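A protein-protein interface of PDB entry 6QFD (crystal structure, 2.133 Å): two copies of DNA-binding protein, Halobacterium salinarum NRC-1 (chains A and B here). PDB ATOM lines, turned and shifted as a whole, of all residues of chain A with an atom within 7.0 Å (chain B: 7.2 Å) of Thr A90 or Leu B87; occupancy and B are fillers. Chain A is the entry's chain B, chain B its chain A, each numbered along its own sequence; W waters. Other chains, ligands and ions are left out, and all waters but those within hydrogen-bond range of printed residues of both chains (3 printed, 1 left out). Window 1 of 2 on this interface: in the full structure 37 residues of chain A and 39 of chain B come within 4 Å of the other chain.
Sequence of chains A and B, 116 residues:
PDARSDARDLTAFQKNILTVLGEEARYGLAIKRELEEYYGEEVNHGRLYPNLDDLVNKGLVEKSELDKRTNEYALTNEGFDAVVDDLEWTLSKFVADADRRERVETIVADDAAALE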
ATOM      1  N   VAL A  84      -6.653  23.797  24.914  1.00  0.00           N
ATOM      2  CA  VAL A  84      -7.127  22.783  25.850  1.00  0.00           C
ATOM      3  C   VAL A  84      -8.574  22.421  25.546  1.00  0.00           C
ATOM      4  O   VAL A  84      -8.940  21.242  25.490  1.00  0.00           O
ATOM      5  CB  VAL A  84      -6.959  23.277  27.298  1.00  0.00           C
ATOM      6  CG1 VAL A  84      -7.638  22.327  28.271  1.00  0.00           C
ATOM      7  CG2 VAL A  84      -5.485  23.430  27.635  1.00  0.00           C
ATOM      8  N   ASP A  85      -9.418  23.434  25.335  1.00  0.00           N
ATOM      9  CA  ASP A  85     -10.830  23.183  25.068  1.00  0.00           C
ATOM     10  C   ASP A  85     -11.017  22.313  23.832  1.00  0.00           C
ATOM     11  O   ASP A  85     -11.842  21.392  23.834  1.00  0.00           O
ATOM     12  CB  ASP A  85     -11.572  24.510  24.905  1.00  0.00           C
ATOM     13  CG  ASP A  85     -11.705  25.271  26.213  1.00  0.00           C
ATOM     14  OD1 ASP A  85     -11.456  24.670  27.281  1.00  0.00           O
ATOM     15  OD2 ASP A  85     -12.057  26.470  26.172  1.00  0.00           O
ATOM     16  N   ASP A  86     -10.267  22.589  22.764  1.00  0.00           N
ATOM     17  CA  ASP A  86     -10.384  21.776  21.557  1.00  0.00           C
ATOM     18  C   ASP A  86      -9.944  20.342  21.819  1.00  0.00           C
ATOM     19  O   ASP A  86     -10.526  19.395  21.272  1.00  0.00           O
ATOM     20  CB  ASP A  86      -9.560  22.387  20.426  1.00  0.00           C
ATOM     21  CG  ASP A  86      -9.666  21.595  19.136  1.00  0.00           C
ATOM     22  OD1 ASP A  86     -10.765  21.572  18.537  1.00  0.00           O
ATOM     23  OD2 ASP A  86      -8.651  20.992  18.723  1.00  0.00           O
ATOM     24  N   LEU A  87      -8.916  20.155  22.649  1.00  0.00           N
ATOM     25  CA  LEU A  87      -8.452  18.805  22.941  1.00  0.00           C
ATOM     26  C   LEU A  87      -9.452  18.057  23.816  1.00  0.00           C
ATOM     27  O   LEU A  87      -9.665  16.853  23.632  1.00  0.00           O
ATOM     28  CB  LEU A  87      -7.080  18.854  23.609  1.00  0.00           C
ATOM     29  CG  LEU A  87      -6.545  17.532  24.160  1.00  0.00           C
ATOM     30  CD1 LEU A  87      -6.107  16.611  23.033  1.00  0.00           C
ATOM     31  CD2 LEU A  87      -5.399  17.785  25.124  1.00  0.00           C
ATOM     32  N   GLU A  88     -10.088  18.753  24.762  1.00  0.00           N
ATOM     33  CA  GLU A  88     -11.079  18.097  25.610  1.00  0.00           C
ATOM     34  C   GLU A  88     -12.304  17.669  24.813  1.00  0.00           C
ATOM     35  O   GLU A  88     -12.940  16.662  25.150  1.00  0.00           O
ATOM     36  CB  GLU A  88     -11.484  19.021  26.759  1.00  0.00           C
ATOM     37  CG  GLU A  88     -10.409  19.172  27.825  1.00  0.00           C
ATOM     38  CD  GLU A  88     -10.808  20.119  28.943  1.00  0.00           C
ATOM     39  OE1 GLU A  88     -10.009  20.293  29.889  1.00  0.00           O
ATOM     40  OE2 GLU A  88     -11.917  20.689  28.875  1.00  0.00           O
ATOM     41  N   TRP A  89     -12.651  18.412  23.758  1.00  0.00           N
ATOM     42  CA  TRP A  89     -13.770  18.027  22.906  1.00  0.00           C
ATOM     43  C   TRP A  89     -13.402  16.832  22.032  1.00  0.00           C
ATOM     44  O   TRP A  89     -14.160  15.862  21.936  1.00  0.00           O
ATOM     45  CB  TRP A  89     -14.203  19.224  22.054  1.00  0.00           C
ATOM     46  CG  TRP A  89     -14.752  18.871  20.699  1.00  0.00           C
ATOM     47  CD1 TRP A  89     -14.078  18.887  19.512  1.00  0.00           C
ATOM     48  CD2 TRP A  89     -16.095  18.468  20.393  1.00  0.00           C
ATOM     49  NE1 TRP A  89     -14.915  18.513  18.488  1.00  0.00           N
ATOM     50  CE2 TRP A  89     -16.157  18.250  19.001  1.00  0.00           C
ATOM     51  CE3 TRP A  89     -17.246  18.268  21.159  1.00  0.00           C
ATOM     52  CZ2 TRP A  89     -17.326  17.841  18.361  1.00  0.00           C
ATOM     53  CZ3 TRP A  89     -18.406  17.860  20.521  1.00  0.00           C
ATOM     54  CH2 TRP A  89     -18.436  17.653  19.137  1.00  0.00           C
ATOM     55  N   THR A  90     -12.229  16.887  21.398  1.00  0.00           N
ATOM     56  CA  THR A  90     -11.763  15.762  20.592  1.00  0.00           C
ATOM     57  C   THR A  90     -11.712  14.489  21.422  1.00  0.00           C
ATOM     58  O   THR A  90     -12.170  13.426  20.985  1.00  0.00           O
ATOM     59  CB  THR A  90     -10.384  16.083  20.006  1.00  0.00           C
ATOM     60  OG1 THR A  90     -10.519  17.065  18.969  1.00  0.00           O
ATOM     61  CG2 THR A  90      -9.730  14.832  19.432  1.00  0.00           C
ATOM     62  N   LEU A  91     -11.172  14.582  22.641  1.00  0.00           N
ATOM     63  CA  LEU A  91     -11.042  13.401  23.486  1.00  0.00           C
ATOM     64  C   LEU A  91     -12.401  12.913  23.972  1.00  0.00           C
ATOM     65  O   LEU A  91     -12.662  11.704  23.989  1.00  0.00           O
ATOM     66  CB  LEU A  91     -10.127  13.708  24.673  1.00  0.00           C
ATOM     67  CG  LEU A  91      -8.631  13.829  24.374  1.00  0.00           C
ATOM     68  CD1 LEU A  91      -7.860  14.243  25.619  1.00  0.00           C
ATOM     69  CD2 LEU A  91      -8.092  12.522  23.827  1.00  0.00           C
ATOM     70  N   SER A  92     -13.279  13.836  24.372  1.00  0.00           N
ATOM     71  CA  SER A  92     -14.594  13.437  24.865  1.00  0.00           C
ATOM     72  C   SER A  92     -15.349  12.604  23.840  1.00  0.00           C
ATOM     73  O   SER A  92     -16.200  11.788  24.210  1.00  0.00           O
ATOM     74  CB  SER A  92     -15.417  14.670  25.237  1.00  0.00           C
ATOM     75  OG  SER A  92     -15.876  15.338  24.073  1.00  0.00           O
ATOM     76  N   LYS A  93     -15.061  12.798  22.554  1.00  0.00           N
ATOM     77  CA  LYS A  93     -15.690  12.007  21.506  1.00  0.00           C
ATOM     78  C   LYS A  93     -14.857  10.802  21.097  1.00  0.00           C
ATOM     79  O   LYS A  93     -15.414   9.832  20.570  1.00  0.00           O
ATOM     80  CB  LYS A  93     -15.956  12.880  20.276  1.00  0.00           C
ATOM     81  CG  LYS A  93     -16.969  13.989  20.516  1.00  0.00           C
ATOM     82  CD  LYS A  93     -18.369  13.425  20.716  1.00  0.00           C
ATOM     83  CE  LYS A  93     -19.415  14.524  20.809  1.00  0.00           C
ATOM     84  NZ  LYS A  93     -19.473  15.121  22.174  1.00  0.00           N
ATOM     85  N   PHE A  94     -13.544  10.832  21.330  1.00  0.00           N
ATOM     86  CA  PHE A  94     -12.693   9.712  20.945  1.00  0.00           C
ATOM     87  C   PHE A  94     -12.681   8.622  22.011  1.00  0.00           C
ATOM     88  O   PHE A  94     -12.732   7.430  21.684  1.00  0.00           O
ATOM     89  CB  PHE A  94     -11.270  10.206  20.677  1.00  0.00           C
ATOM     90  CG  PHE A  94     -10.350   9.140  20.155  1.00  0.00           C
ATOM     91  CD1 PHE A  94     -10.310   8.845  18.803  1.00  0.00           C
ATOM     92  CD2 PHE A  94      -9.528   8.433  21.014  1.00  0.00           C
ATOM     93  CE1 PHE A  94      -9.467   7.864  18.317  1.00  0.00           C
ATOM     94  CE2 PHE A  94      -8.683   7.452  20.536  1.00  0.00           C
ATOM     95  CZ  PHE A  94      -8.652   7.166  19.185  1.00  0.00           C
ATOM     96  N   VAL A  95     -12.611   9.004  23.286  1.00  0.00           N
ATOM     97  CA  VAL A  95     -12.581   8.032  24.373  1.00  0.00           C
ATOM     98  C   VAL A  95     -13.977   7.450  24.543  1.00  0.00           C
ATOM     99  O   VAL A  95     -14.720   7.838  25.451  1.00  0.00           O
ATOM    100  CB  VAL A  95     -12.079   8.666  25.683  1.00  0.00           C
ATOM    101  CG1 VAL A  95     -12.005   7.618  26.783  1.00  0.00           C
ATOM    102  CG2 VAL A  95     -10.719   9.316  25.470  1.00  0.00           C
ATOM    103  N   ARG A 100     -10.172   2.560  23.061  1.00  0.00           N
ATOM    104  CA  ARG A 100      -9.885   3.934  22.669  1.00  0.00           C
ATOM    105  C   ARG A 100      -9.040   4.639  23.720  1.00  0.00           C
ATOM    106  O   ARG A 100      -8.108   5.380  23.388  1.00  0.00           O
ATOM    107  CB  ARG A 100     -11.188   4.696  22.448  1.00  0.00           C
ATOM    108  CG  ARG A 100     -11.981   4.217  21.255  1.00  0.00           C
ATOM    109  CD  ARG A 100     -11.398   4.761  19.966  1.00  0.00           C
ATOM    110  NE  ARG A 100     -12.282   4.517  18.831  1.00  0.00           N
ATOM    111  CZ  ARG A 100     -13.352   5.251  18.544  1.00  0.00           C
ATOM    112  NH1 ARG A 100     -13.683   6.284  19.306  1.00  0.00           N
ATOM    113  NH2 ARG A 100     -14.095   4.947  17.490  1.00  0.00           N
ATOM    114  N   ARG A 103      -5.404   3.470  23.804  1.00  0.00           N
ATOM    115  CA  ARG A 103      -4.755   3.997  22.641  1.00  0.00           C
ATOM    116  C   ARG A 103      -4.235   5.372  22.930  1.00  0.00           C
ATOM    117  O   ARG A 103      -3.095   5.679  22.618  1.00  0.00           O
ATOM    118  CB  ARG A 103      -5.686   4.042  21.442  1.00  0.00           C
ATOM    119  CG  ARG A 103      -5.107   4.886  20.336  1.00  0.00           C
ATOM    120  CD  ARG A 103      -6.061   4.900  19.206  1.00  0.00           C
ATOM    121  NE  ARG A 103      -5.619   4.064  18.123  1.00  0.00           N
ATOM    122  CZ  ARG A 103      -6.219   2.944  17.784  1.00  0.00           C
ATOM    123  NH1 ARG A 103      -7.252   2.511  18.482  1.00  0.00           N
ATOM    124  NH2 ARG A 103      -5.759   2.259  16.766  1.00  0.00           N
ATOM    125  N   VAL A 104      -5.058   6.251  23.528  1.00  0.00           N
ATOM    126  CA  VAL A 104      -4.604   7.591  23.891  1.00  0.00           C
ATOM    127  C   VAL A 104      -3.466   7.510  24.896  1.00  0.00           C
ATOM    128  O   VAL A 104      -2.510   8.294  24.845  1.00  0.00           O
ATOM    129  CB  VAL A 104      -5.783   8.414  24.448  1.00  0.00           C
ATOM    130  CG1 VAL A 104      -5.322   9.812  24.837  1.00  0.00           C
ATOM    131  CG2 VAL A 104      -6.911   8.487  23.432  1.00  0.00           C
ATOM    132  N   ILE A 107      -0.226   6.774  23.180  1.00  0.00           N
ATOM    133  CA  ILE A 107       0.185   7.980  22.466  1.00  0.00           C
ATOM    134  C   ILE A 107       0.852   8.957  23.429  1.00  0.00           C
ATOM    135  O   ILE A 107       1.945   9.469  23.167  1.00  0.00           O
ATOM    136  CB  ILE A 107      -1.017   8.633  21.761  1.00  0.00           C
ATOM    137  CG1 ILE A 107      -1.575   7.718  20.671  1.00  0.00           C
ATOM    138  CG2 ILE A 107      -0.606   9.978  21.171  1.00  0.00           C
ATOM    139  CD1 ILE A 107      -2.905   8.192  20.101  1.00  0.00           C
ATOM    140  N   ASP A 111       4.798  10.138  23.560  1.00  0.00           N
ATOM    141  CA  ASP A 111       5.150  11.551  23.480  1.00  0.00           C
ATOM    142  C   ASP A 111       6.058  11.956  24.634  1.00  0.00           C
ATOM    143  O   ASP A 111       7.044  12.674  24.435  1.00  0.00           O
ATOM    144  CB  ASP A 111       3.884  12.407  23.471  1.00  0.00           C
ATOM    145  CG  ASP A 111       3.080  12.247  22.195  1.00  0.00           C
ATOM    146  OD1 ASP A 111       3.658  11.814  21.177  1.00  0.00           O
ATOM    147  OD2 ASP A 111       1.870  12.559  22.210  1.00  0.00           O
ATOM    148  N   LYS B  15     -13.784  17.848   9.874  1.00  0.00           N
ATOM    149  CA  LYS B  15     -13.145  17.103  10.956  1.00  0.00           C
ATOM    150  C   LYS B  15     -14.068  16.999  12.157  1.00  0.00           C
ATOM    151  O   LYS B  15     -14.071  15.983  12.861  1.00  0.00           O
ATOM    152  CB  LYS B  15     -11.832  17.787  11.345  1.00  0.00           C
ATOM    153  CG  LYS B  15     -10.935  16.918  12.224  1.00  0.00           C
ATOM    154  CD  LYS B  15     -10.928  17.389  13.675  1.00  0.00           C
ATOM    155  CE  LYS B  15      -9.719  16.855  14.435  1.00  0.00           C
ATOM    156  NZ  LYS B  15      -9.314  17.763  15.544  1.00  0.00           N
ATOM    157  N   ASN B  16     -14.865  18.041  12.406  1.00  0.00           N
ATOM    158  CA  ASN B  16     -15.861  17.974  13.469  1.00  0.00           C
ATOM    159  C   ASN B  16     -16.890  16.884  13.183  1.00  0.00           C
ATOM    160  O   ASN B  16     -17.374  16.222  14.105  1.00  0.00           O
ATOM    161  CB  ASN B  16     -16.544  19.331  13.632  1.00  0.00           C
ATOM    162  CG  ASN B  16     -15.651  20.355  14.308  1.00  0.00           C
ATOM    163  OD1 ASN B  16     -14.694  20.001  14.997  1.00  0.00           O
ATOM    164  ND2 ASN B  16     -15.963  21.632  14.116  1.00  0.00           N
ATOM    165  N   THR B  19     -15.067  13.692  14.061  1.00  0.00           N
ATOM    166  CA  THR B  19     -14.995  13.572  15.513  1.00  0.00           C
ATOM    167  C   THR B  19     -16.323  13.084  16.073  1.00  0.00           C
ATOM    168  O   THR B  19     -16.363  12.186  16.923  1.00  0.00           O
ATOM    169  CB  THR B  19     -14.610  14.909  16.145  1.00  0.00           C
ATOM    170  OG1 THR B  19     -13.361  15.358  15.608  1.00  0.00           O
ATOM    171  CG2 THR B  19     -14.487  14.764  17.657  1.00  0.00           C
ATOM    172  N   TYR B  38     -22.238  21.866  19.589  1.00  0.00           N
ATOM    173  CA  TYR B  38     -20.835  22.259  19.628  1.00  0.00           C
ATOM    174  C   TYR B  38     -20.670  23.726  19.250  1.00  0.00           C
ATOM    175  O   TYR B  38     -20.090  24.516  20.004  1.00  0.00           O
ATOM    176  CB  TYR B  38     -20.021  21.368  18.689  1.00  0.00           C
ATOM    177  CG  TYR B  38     -18.599  21.838  18.491  1.00  0.00           C
ATOM    178  CD1 TYR B  38     -17.605  21.495  19.392  1.00  0.00           C
ATOM    179  CD2 TYR B  38     -18.254  22.630  17.403  1.00  0.00           C
ATOM    180  CE1 TYR B  38     -16.304  21.924  19.218  1.00  0.00           C
ATOM    181  CE2 TYR B  38     -16.956  23.065  17.220  1.00  0.00           C
ATOM    182  CZ  TYR B  38     -15.985  22.711  18.131  1.00  0.00           C
ATOM    183  OH  TYR B  38     -14.689  23.140  17.951  1.00  0.00           O
ATOM    184  N   ASP B  81      -8.489   6.351  10.885  1.00  0.00           N
ATOM    185  CA  ASP B  81      -7.063   6.661  10.851  1.00  0.00           C
ATOM    186  C   ASP B  81      -6.824   8.157  10.703  1.00  0.00           C
ATOM    187  O   ASP B  81      -5.851   8.687  11.250  1.00  0.00           O
ATOM    188  CB  ASP B  81      -6.387   5.898   9.711  1.00  0.00           C
ATOM    189  CG  ASP B  81      -6.176   4.429  10.033  1.00  0.00           C
ATOM    190  OD1 ASP B  81      -6.934   3.884  10.864  1.00  0.00           O
ATOM    191  OD2 ASP B  81      -5.253   3.817   9.453  1.00  0.00           O
ATOM    192  N   ALA B  82      -7.695   8.853   9.969  1.00  0.00           N
ATOM    193  CA  ALA B  82      -7.599  10.306   9.889  1.00  0.00           C
ATOM    194  C   ALA B  82      -7.824  10.936  11.258  1.00  0.00           C
ATOM    195  O   ALA B  82      -7.064  11.812  11.685  1.00  0.00           O
ATOM    196  CB  ALA B  82      -8.609  10.843   8.875  1.00  0.00           C
ATOM    197  N   VAL B  83      -8.869  10.495  11.961  1.00  0.00           N
ATOM    198  CA  VAL B  83      -9.141  11.013  13.300  1.00  0.00           C
ATOM    199  C   VAL B  83      -7.949  10.763  14.215  1.00  0.00           C
ATOM    200  O   VAL B  83      -7.505  11.656  14.946  1.00  0.00           O
ATOM    201  CB  VAL B  83     -10.425  10.381  13.866  1.00  0.00           C
ATOM    202  CG1 VAL B  83     -10.554  10.670  15.357  1.00  0.00           C
ATOM    203  CG2 VAL B  83     -11.644  10.886  13.112  1.00  0.00           C
ATOM    204  N   VAL B  84      -7.410   9.543  14.186  1.00  0.00           N
ATOM    205  CA  VAL B  84      -6.324   9.194  15.096  1.00  0.00           C
ATOM    206  C   VAL B  84      -5.077  10.008  14.782  1.00  0.00           C
ATOM    207  O   VAL B  84      -4.342  10.417  15.688  1.00  0.00           O
ATOM    208  CB  VAL B  84      -6.036   7.683  15.037  1.00  0.00           C
ATOM    209  CG1 VAL B  84      -4.740   7.366  15.769  1.00  0.00           C
ATOM    210  CG2 VAL B  84      -7.194   6.893  15.628  1.00  0.00           C
ATOM    211  N   ASP B  85      -4.811  10.256  13.499  1.00  0.00           N
ATOM    212  CA  ASP B  85      -3.601  10.982  13.130  1.00  0.00           C
ATOM    213  C   ASP B  85      -3.652  12.423  13.622  1.00  0.00           C
ATOM    214  O   ASP B  85      -2.671  12.932  14.175  1.00  0.00           O
ATOM    215  CB  ASP B  85      -3.395  10.934  11.618  1.00  0.00           C
ATOM    216  CG  ASP B  85      -2.038  11.467  11.200  1.00  0.00           C
ATOM    217  OD1 ASP B  85      -1.074  10.674  11.159  1.00  0.00           O
ATOM    218  OD2 ASP B  85      -1.938  12.680  10.920  1.00  0.00           O
ATOM    219  N   ASP B  86      -4.786  13.102  13.424  1.00  0.00           N
ATOM    220  CA  ASP B  86      -4.922  14.465  13.930  1.00  0.00           C
ATOM    221  C   ASP B  86      -4.807  14.494  15.450  1.00  0.00           C
ATOM    222  O   ASP B  86      -4.169  15.390  16.016  1.00  0.00           O
ATOM    223  CB  ASP B  86      -6.255  15.066  13.480  1.00  0.00           C
ATOM    224  CG  ASP B  86      -6.165  15.739  12.117  1.00  0.00           C
ATOM    225  OD1 ASP B  86      -5.045  16.094  11.692  1.00  0.00           O
ATOM    226  OD2 ASP B  86      -7.221  15.916  11.469  1.00  0.00           O
ATOM    227  N   LEU B  87      -5.421  13.517  16.125  1.00  0.00           N
ATOM    228  CA  LEU B  87      -5.259  13.379  17.570  1.00  0.00           C
ATOM    229  C   LEU B  87      -3.793  13.244  17.943  1.00  0.00           C
ATOM    230  O   LEU B  87      -3.333  13.835  18.933  1.00  0.00           O
ATOM    231  CB  LEU B  87      -6.049  12.163  18.059  1.00  0.00           C
ATOM    232  CG  LEU B  87      -5.845  11.726  19.511  1.00  0.00           C
ATOM    233  CD1 LEU B  87      -6.517  12.693  20.471  1.00  0.00           C
ATOM    234  CD2 LEU B  87      -6.370  10.313  19.717  1.00  0.00           C
ATOM    235  N   GLU B  88      -3.043  12.450  17.174  1.00  0.00           N
ATOM    236  CA  GLU B  88      -1.635  12.235  17.472  1.00  0.00           C
ATOM    237  C   GLU B  88      -0.828  13.512  17.279  1.00  0.00           C
ATOM    238  O   GLU B  88       0.106  13.783  18.043  1.00  0.00           O
ATOM    239  CB  GLU B  88      -1.074  11.115  16.595  1.00  0.00           C
ATOM    240  CG  GLU B  88      -1.471   9.719  17.048  1.00  0.00           C
ATOM    241  CD  GLU B  88      -0.938   8.634  16.132  1.00  0.00           C
ATOM    242  OE1 GLU B  88      -0.422   8.969  15.043  1.00  0.00           O
ATOM    243  OE2 GLU B  88      -1.036   7.445  16.502  1.00  0.00           O
ATOM    244  N   TRP B  89      -1.167  14.311  16.265  1.00  0.00           N
ATOM    245  CA  TRP B  89      -0.413  15.536  16.022  1.00  0.00           C
ATOM    246  C   TRP B  89      -0.671  16.562  17.118  1.00  0.00           C
ATOM    247  O   TRP B  89       0.271  17.144  17.668  1.00  0.00           O
ATOM    248  CB  TRP B  89      -0.759  16.118  14.653  1.00  0.00           C
ATOM    249  CG  TRP B  89       0.165  17.233  14.272  1.00  0.00           C
ATOM    250  CD1 TRP B  89       1.493  17.129  13.977  1.00  0.00           C
ATOM    251  CD2 TRP B  89      -0.161  18.624  14.168  1.00  0.00           C
ATOM    252  NE1 TRP B  89       2.013  18.367  13.690  1.00  0.00           N
ATOM    253  CE2 TRP B  89       1.018  19.301  13.798  1.00  0.00           C
ATOM    254  CE3 TRP B  89      -1.336  19.361  14.347  1.00  0.00           C
ATOM    255  CZ2 TRP B  89       1.056  20.679  13.604  1.00  0.00           C
ATOM    256  CZ3 TRP B  89      -1.295  20.730  14.153  1.00  0.00           C
ATOM    257  CH2 TRP B  89      -0.107  21.374  13.786  1.00  0.00           C
ATOM    258  N   THR B  90      -1.942  16.804  17.447  1.00  0.00           N
ATOM    259  CA  THR B  90      -2.254  17.746  18.518  1.00  0.00           C
ATOM    260  C   THR B  90      -1.573  17.333  19.817  1.00  0.00           C
ATOM    261  O   THR B  90      -0.977  18.168  20.509  1.00  0.00           O
ATOM    262  CB  THR B  90      -3.768  17.846  18.716  1.00  0.00           C
ATOM    263  OG1 THR B  90      -4.312  16.542  18.954  1.00  0.00           O
ATOM    264  CG2 THR B  90      -4.435  18.459  17.487  1.00  0.00           C
ATOM    265  N   LEU B  91      -1.633  16.044  20.155  1.00  0.00           N
ATOM    266  CA  LEU B  91      -0.995  15.572  21.378  1.00  0.00           C
ATOM    267  C   LEU B  91       0.522  15.685  21.293  1.00  0.00           C
ATOM    268  O   LEU B  91       1.180  16.033  22.279  1.00  0.00           O
ATOM    269  CB  LEU B  91      -1.407  14.129  21.662  1.00  0.00           C
ATOM    270  CG  LEU B  91      -2.839  13.924  22.158  1.00  0.00           C
ATOM    271  CD1 LEU B  91      -3.183  12.444  22.178  1.00  0.00           C
ATOM    272  CD2 LEU B  91      -3.033  14.537  23.535  1.00  0.00           C
ATOM    273  N   SER B  92       1.097  15.386  20.123  1.00  0.00           N
ATOM    274  CA  SER B  92       2.544  15.481  19.970  1.00  0.00           C
ATOM    275  C   SER B  92       3.045  16.881  20.283  1.00  0.00           C
ATOM    276  O   SER B  92       4.166  17.049  20.771  1.00  0.00           O
ATOM    277  CB  SER B  92       2.954  15.082  18.552  1.00  0.00           C
ATOM    278  OG  SER B  92       2.874  16.183  17.663  1.00  0.00           O
ATOM    279  N   LYS B  93       2.216  17.896  20.044  1.00  0.00           N
ATOM    280  CA  LYS B  93       2.610  19.267  20.275  1.00  0.00           C
ATOM    281  C   LYS B  93       2.088  19.784  21.587  1.00  0.00           C
ATOM    282  O   LYS B  93       2.586  20.785  22.069  1.00  0.00           O
ATOM    283  CB  LYS B  93       2.137  20.165  19.119  1.00  0.00           C
ATOM    284  CG  LYS B  93       2.791  19.823  17.794  1.00  0.00           C
ATOM    285  CD  LYS B  93       3.960  20.694  17.477  1.00  0.00           C
ATOM    286  CE  LYS B  93       4.740  20.195  16.286  1.00  0.00           C
ATOM    287  NZ  LYS B  93       4.262  20.812  15.030  1.00  0.00           N
ATOM    288  N   ASP B 111     -12.932  11.410  31.195  1.00  0.00           N
ATOM    289  CA  ASP B 111     -13.684  10.863  30.073  1.00  0.00           C
ATOM    290  C   ASP B 111     -14.042   9.395  30.326  1.00  0.00           C
ATOM    291  O   ASP B 111     -15.191   9.010  30.140  1.00  0.00           O
ATOM    292  CB  ASP B 111     -12.881  10.973  28.777  1.00  0.00           C
ATOM    293  CG  ASP B 111     -12.821  12.373  28.211  1.00  0.00           C
ATOM    294  OD1 ASP B 111     -13.485  13.279  28.710  1.00  0.00           O
ATOM    295  OD2 ASP B 111     -12.069  12.553  27.245  1.00  0.00           O
HETATM  296  O   HOH W   1       1.600  11.987  19.425  1.00  0.00           O
HETATM  297  O   HOH W   2     -13.889  10.880  17.992  1.00  0.00           O
HETATM  298  O   HOH W   3     -12.738  15.317  27.216  1.00  0.00           O
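The side-chain hydroxyl (OG1) of Thr B19 is in hydrogen-bond range of the backbone carbonyl oxygen (O) of Lys B15, 2.9 Å away.
The backbone carbonyl oxygen of Trp B89 sits at hydrogen-bond distance from the side-chain hydroxyl of Ser B92.
The backbone carbonyl oxygen (O) of Trp A89 is in hydrogen-bond range of the side-chain hydroxyl (OG) of Ser A92.
O of Leu B87 is in hydrogen-bond range of OG1 of Thr B90, 2.9 Å away.
O of Phe A94 lies within hydrogen-bond range of NH1 of Arg A100 (2.8 Å).
The side-chain hydroxyl (OG1) of Thr A90 sits at hydrogen-bond distance from the backbone carbonyl oxygen (O) of Asp A86.
Printed residues of chain B that touch a printed residue of chain A: Lys B15, Asn B16, Thr B19, Tyr B38, Val B83, Val B84, Leu B87, Glu B88, Leu B91, Ser B92 and Asp B111.
Printed residues of chain A that touch a printed residue of chain B: Leu A87, Trp A89, Thr A90, Leu A91, Ser A92, Lys A93, Phe A94, Val A95, Ile A107 and Asp A111.
Of the printed residues of chain B, Thr A90 touches Lys B15 and Leu B87.
Of the printed residues of chain B, Ser A92 touches Asp B111.
Printed residues of chain A within 4 Å of Leu B87: Thr A90 (3.997 Å), Leu A91 (3.7 Å) and Phe A94 (3.8 Å).
Of the printed residues of chain A, Ser B92 touches Asp A111.
Lys B93 touches none of the printed residues of chain A.
The nearest printed residue of chain B that does not touch Thr A90 is Thr B19 (4.1 Å).
Among the printed residues, merely in contact across the chains: Leu A87 with Leu B91, Trp A89 with Asn B16, Trp A89 with Thr B19, Trp A89 with Tyr B38, Thr A90 with Lys B15, Thr A90 with Leu B87, Leu A91 with Leu B87, Lys A93 with Thr B19, Phe A94 with Val B83, Phe A94 with Val B84, Phe A94 with Leu B87, Val A95 with Asp B111, Ile A107 with Glu B88, Ile A107 with Leu B91, Asp A111 with Leu B91 and Asp A111 with Ser B92.
Water W3 lies within hydrogen-bond range of the backbone carbonyl oxygen (O) of Glu A88 (2.5 Å), the side-chain carboxylate (OD1) of Asp B111 (2.6 Å) and the backbone NH (N) of Ser A92 (3.3 Å).
Water W1 bridges OD1 of Asp A111 and O of Glu B88.
Water W2 lies within hydrogen-bond range of the backbone carbonyl oxygen of Thr B19 (3.0 Å), the backbone carbonyl oxygen of Lys A93 (3.2 Å) and the backbone NH of Phe A94 (3.4 Å).
The side-chain carboxylate (OD2) of Asp B111 lies close to the backbone carbonyl oxygen (O) of Leu A91 (3.4 Å).
The side-chain carboxylate of Asp B111 lies within hydrogen-bond range of the backbone NH of Ser A92.
Leu A87 touches Leu B91, and with the chains exchanged Leu A91 touches Leu B87.
Thr A90 touches Leu B87, but with the chains exchanged Leu A87 does not touch Thr B90 (4.5 Å).
Leu A91 touches Asp B111, and with the chains exchanged Asp A111 touches Leu B91.
Ser A92 touches Asp B111, and with the chains exchanged Asp A111 touches Ser B92.
11 positions are printed for both chains.
Of the 18 pairs that touch across the chains among the printed residues, 6 have their exchanged pair printed and touching as well.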
